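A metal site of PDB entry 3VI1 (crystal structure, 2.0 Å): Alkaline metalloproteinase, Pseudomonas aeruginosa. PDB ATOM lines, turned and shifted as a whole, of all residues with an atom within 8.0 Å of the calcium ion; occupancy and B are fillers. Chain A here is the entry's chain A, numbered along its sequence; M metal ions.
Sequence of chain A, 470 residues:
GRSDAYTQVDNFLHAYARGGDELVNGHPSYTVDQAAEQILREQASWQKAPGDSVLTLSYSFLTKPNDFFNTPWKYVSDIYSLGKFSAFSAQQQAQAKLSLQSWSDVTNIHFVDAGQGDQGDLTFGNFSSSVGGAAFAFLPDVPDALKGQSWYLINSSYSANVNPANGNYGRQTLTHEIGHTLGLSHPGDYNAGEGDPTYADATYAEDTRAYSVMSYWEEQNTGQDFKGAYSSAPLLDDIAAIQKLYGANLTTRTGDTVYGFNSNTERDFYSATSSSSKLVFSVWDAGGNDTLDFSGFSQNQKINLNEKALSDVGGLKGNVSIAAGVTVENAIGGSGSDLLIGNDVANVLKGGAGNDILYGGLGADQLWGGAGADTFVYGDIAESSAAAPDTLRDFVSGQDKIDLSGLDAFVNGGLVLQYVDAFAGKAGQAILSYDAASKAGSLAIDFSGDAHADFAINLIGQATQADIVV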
ATOM      1  N   ALA A 386     -10.039  23.100   9.605  1.00  0.00           N
ATOM      2  CA  ALA A 386      -8.659  23.581   9.559  1.00  0.00           C
ATOM      3  C   ALA A 386      -7.976  23.534  10.934  1.00  0.00           C
ATOM      4  O   ALA A 386      -6.758  23.382  11.015  1.00  0.00           O
ATOM      5  CB  ALA A 386      -8.599  24.988   8.993  1.00  0.00           C
ATOM      6  N   PHE A 423      -2.432  32.108   0.199  1.00  0.00           N
ATOM      7  CA  PHE A 423      -3.804  32.503  -0.102  1.00  0.00           C
ATOM      8  C   PHE A 423      -3.912  34.004  -0.383  1.00  0.00           C
ATOM      9  O   PHE A 423      -3.548  34.841   0.461  1.00  0.00           O
ATOM     10  CB  PHE A 423      -4.753  32.115   1.042  1.00  0.00           C
ATOM     11  CG  PHE A 423      -4.932  30.626   1.210  1.00  0.00           C
ATOM     12  CD1 PHE A 423      -5.027  29.785   0.103  1.00  0.00           C
ATOM     13  CD2 PHE A 423      -5.042  30.074   2.482  1.00  0.00           C
ATOM     14  CE1 PHE A 423      -5.197  28.417   0.269  1.00  0.00           C
ATOM     15  CE2 PHE A 423      -5.216  28.700   2.655  1.00  0.00           C
ATOM     16  CZ  PHE A 423      -5.297  27.875   1.542  1.00  0.00           C
ATOM     17  N   LYS A 426      -9.018  34.022  -2.642  1.00  0.00           N
ATOM     18  CA  LYS A 426      -9.782  33.459  -3.747  1.00  0.00           C
ATOM     19  C   LYS A 426     -10.342  32.088  -3.378  1.00  0.00           C
ATOM     20  O   LYS A 426      -9.642  31.252  -2.796  1.00  0.00           O
ATOM     21  CB  LYS A 426      -8.902  33.359  -5.005  1.00  0.00           C
ATOM     22  CG  LYS A 426      -9.601  32.789  -6.230  1.00  0.00           C
ATOM     23  CD  LYS A 426      -8.718  32.880  -7.469  1.00  0.00           C
ATOM     24  CE  LYS A 426      -9.258  32.007  -8.600  1.00  0.00           C
ATOM     25  NZ  LYS A 426     -10.598  32.431  -9.084  1.00  0.00           N
ATOM     26  N   ALA A 427     -11.615  31.871  -3.716  1.00  0.00           N
ATOM     27  CA  ALA A 427     -12.297  30.613  -3.458  1.00  0.00           C
ATOM     28  C   ALA A 427     -11.700  29.471  -4.267  1.00  0.00           C
ATOM     29  O   ALA A 427     -11.530  29.572  -5.482  1.00  0.00           O
ATOM     30  CB  ALA A 427     -13.782  30.751  -3.743  1.00  0.00           C
ATOM     31  N   ILE A 445      -7.334  23.926   2.292  1.00  0.00           N
ATOM     32  CA  ILE A 445      -8.097  24.604   1.237  1.00  0.00           C
ATOM     33  C   ILE A 445      -8.923  25.775   1.800  1.00  0.00           C
ATOM     34  O   ILE A 445      -9.520  25.674   2.870  1.00  0.00           O
ATOM     35  CB  ILE A 445      -9.036  23.633   0.473  1.00  0.00           C
ATOM     36  CG1 ILE A 445      -8.293  22.356   0.059  1.00  0.00           C
ATOM     37  CG2 ILE A 445      -9.654  24.320  -0.748  1.00  0.00           C
ATOM     38  CD1 ILE A 445      -9.188  21.217  -0.404  1.00  0.00           C
ATOM     39  N   ASP A 446      -8.913  26.882   1.061  1.00  0.00           N
ATOM     40  CA  ASP A 446      -9.759  28.033   1.355  1.00  0.00           C
ATOM     41  C   ASP A 446     -10.949  28.026   0.393  1.00  0.00           C
ATOM     42  O   ASP A 446     -10.846  28.500  -0.744  1.00  0.00           O
ATOM     43  CB  ASP A 446      -8.941  29.333   1.234  1.00  0.00           C
ATOM     44  CG  ASP A 446      -9.793  30.592   1.363  1.00  0.00           C
ATOM     45  OD1 ASP A 446     -10.870  30.557   2.003  1.00  0.00           O
ATOM     46  OD2 ASP A 446      -9.365  31.631   0.826  1.00  0.00           O
ATOM     47  N   PHE A 447     -12.066  27.470   0.842  1.00  0.00           N
ATOM     48  CA  PHE A 447     -13.270  27.344   0.023  1.00  0.00           C
ATOM     49  C   PHE A 447     -14.085  28.637  -0.081  1.00  0.00           C
ATOM     50  O   PHE A 447     -14.660  28.934  -1.125  1.00  0.00           O
ATOM     51  CB  PHE A 447     -14.161  26.206   0.529  1.00  0.00           C
ATOM     52  CG  PHE A 447     -13.685  24.831   0.117  1.00  0.00           C
ATOM     53  CD1 PHE A 447     -13.881  24.373  -1.182  1.00  0.00           C
ATOM     54  CD2 PHE A 447     -13.065  23.996   1.043  1.00  0.00           C
ATOM     55  CE1 PHE A 447     -13.441  23.112  -1.562  1.00  0.00           C
ATOM     56  CE2 PHE A 447     -12.629  22.729   0.671  1.00  0.00           C
ATOM     57  CZ  PHE A 447     -12.820  22.276  -0.635  1.00  0.00           C
ATOM     58  N   SER A 448     -14.124  29.398   1.017  1.00  0.00           N
ATOM     59  CA  SER A 448     -14.893  30.643   1.064  1.00  0.00           C
ATOM     60  C   SER A 448     -14.200  31.783   0.298  1.00  0.00           C
ATOM     61  O   SER A 448     -14.867  32.592  -0.353  1.00  0.00           O
ATOM     62  CB  SER A 448     -15.151  31.068   2.515  1.00  0.00           C
ATOM     63  OG  SER A 448     -13.930  31.347   3.191  1.00  0.00           O
ATOM     64  N   GLY A 449     -12.873  31.835   0.392  1.00  0.00           N
ATOM     65  CA  GLY A 449     -12.090  32.852  -0.305  1.00  0.00           C
ATOM     66  C   GLY A 449     -11.712  34.048   0.548  1.00  0.00           C
ATOM     67  O   GLY A 449     -11.532  35.149   0.018  1.00  0.00           O
ATOM     68  N   ASP A 450     -11.583  33.840   1.856  1.00  0.00           N
ATOM     69  CA  ASP A 450     -11.195  34.926   2.774  1.00  0.00           C
ATOM     70  C   ASP A 450      -9.714  34.865   3.143  1.00  0.00           C
ATOM     71  O   ASP A 450      -9.294  35.450   4.148  1.00  0.00           O
ATOM     72  CB  ASP A 450     -12.096  34.924   4.026  1.00  0.00           C
ATOM     73  CG  ASP A 450     -11.829  33.748   4.957  1.00  0.00           C
ATOM     74  OD1 ASP A 450     -11.285  32.715   4.505  1.00  0.00           O
ATOM     75  OD2 ASP A 450     -12.173  33.859   6.156  1.00  0.00           O
ATOM     76  N   ALA A 451      -8.931  34.158   2.331  1.00  0.00           N
ATOM     77  CA  ALA A 451      -7.491  33.948   2.532  1.00  0.00           C
ATOM     78  C   ALA A 451      -7.137  33.104   3.756  1.00  0.00           C
ATOM     79  O   ALA A 451      -5.970  33.013   4.146  1.00  0.00           O
ATOM     80  CB  ALA A 451      -6.729  35.295   2.535  1.00  0.00           C
ATOM     81  N   HIS A 452      -8.137  32.476   4.358  1.00  0.00           N
ATOM     82  CA  HIS A 452      -7.949  31.589   5.508  1.00  0.00           C
ATOM     83  C   HIS A 452      -8.458  30.186   5.207  1.00  0.00           C
ATOM     84  O   HIS A 452      -9.476  30.023   4.528  1.00  0.00           O
ATOM     85  CB  HIS A 452      -8.632  32.153   6.749  1.00  0.00           C
ATOM     86  CG  HIS A 452      -8.056  33.442   7.237  1.00  0.00           C
ATOM     87  ND1 HIS A 452      -8.600  34.674   6.915  1.00  0.00           N
ATOM     88  CD2 HIS A 452      -6.979  33.694   8.009  1.00  0.00           C
ATOM     89  CE1 HIS A 452      -7.883  35.621   7.483  1.00  0.00           C
ATOM     90  NE2 HIS A 452      -6.887  35.062   8.145  1.00  0.00           N
ATOM     91  N   ALA A 453      -7.768  29.182   5.728  1.00  0.00           N
ATOM     92  CA  ALA A 453      -8.156  27.788   5.543  1.00  0.00           C
ATOM     93  C   ALA A 453      -9.423  27.458   6.345  1.00  0.00           C
ATOM     94  O   ALA A 453      -9.524  27.808   7.519  1.00  0.00           O
ATOM     95  CB  ALA A 453      -7.022  26.853   5.917  1.00  0.00           C
ATOM     96  N   ASP A 454     -10.366  26.796   5.682  1.00  0.00           N
ATOM     97  CA  ASP A 454     -11.607  26.334   6.332  1.00  0.00           C
ATOM     98  C   ASP A 454     -11.739  24.815   6.254  1.00  0.00           C
ATOM     99  O   ASP A 454     -12.661  24.231   6.815  1.00  0.00           O
ATOM    100  CB  ASP A 454     -12.835  27.025   5.726  1.00  0.00           C
ATOM    101  CG  ASP A 454     -12.781  27.116   4.212  1.00  0.00           C
ATOM    102  OD1 ASP A 454     -12.538  26.088   3.534  1.00  0.00           O
ATOM    103  OD2 ASP A 454     -13.003  28.223   3.687  1.00  0.00           O
ATOM    104  N   PHE A 455     -10.795  24.194   5.544  1.00  0.00           N
ATOM    105  CA  PHE A 455     -10.741  22.750   5.377  1.00  0.00           C
ATOM    106  C   PHE A 455      -9.283  22.302   5.327  1.00  0.00           C
ATOM    107  O   PHE A 455      -8.470  22.922   4.651  1.00  0.00           O
ATOM    108  CB  PHE A 455     -11.482  22.345   4.093  1.00  0.00           C
ATOM    109  CG  PHE A 455     -11.517  20.855   3.847  1.00  0.00           C
ATOM    110  CD1 PHE A 455     -12.420  20.051   4.524  1.00  0.00           C
ATOM    111  CD2 PHE A 455     -10.663  20.274   2.922  1.00  0.00           C
ATOM    112  CE1 PHE A 455     -12.465  18.673   4.298  1.00  0.00           C
ATOM    113  CE2 PHE A 455     -10.687  18.905   2.688  1.00  0.00           C
ATOM    114  CZ  PHE A 455     -11.602  18.103   3.372  1.00  0.00           C
HETATM  115 CA    CA M   1     -11.920  30.455   4.271  1.00  0.00          CA
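The backbone NH of Gly 449 lies close to the side-chain carboxylate of Asp 446 (2.9 Å). The backbone NH of Ala 451 is in hydrogen-bond range of the side-chain carboxylate of Asp 446 (3.0 Å). OD1 of Asp 454 sits at hydrogen-bond distance from N of Phe 447 (3.1 Å). N of Asp 454 sits at hydrogen-bond distance from O of Ile 445 (3.1 Å).
The calcium ion is bound by OD1 of Asp 450 (2.4 Å). OG of Ser 448 binds the calcium ion, 2.4 Å away. O of His 452 is bound to the calcium ion (2.5 Å). OD1 of Asp 446 is bound to the calcium ion, 2.5 Å away. The calcium ion is bound by OD2 of Asp 454 (2.5 Å).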
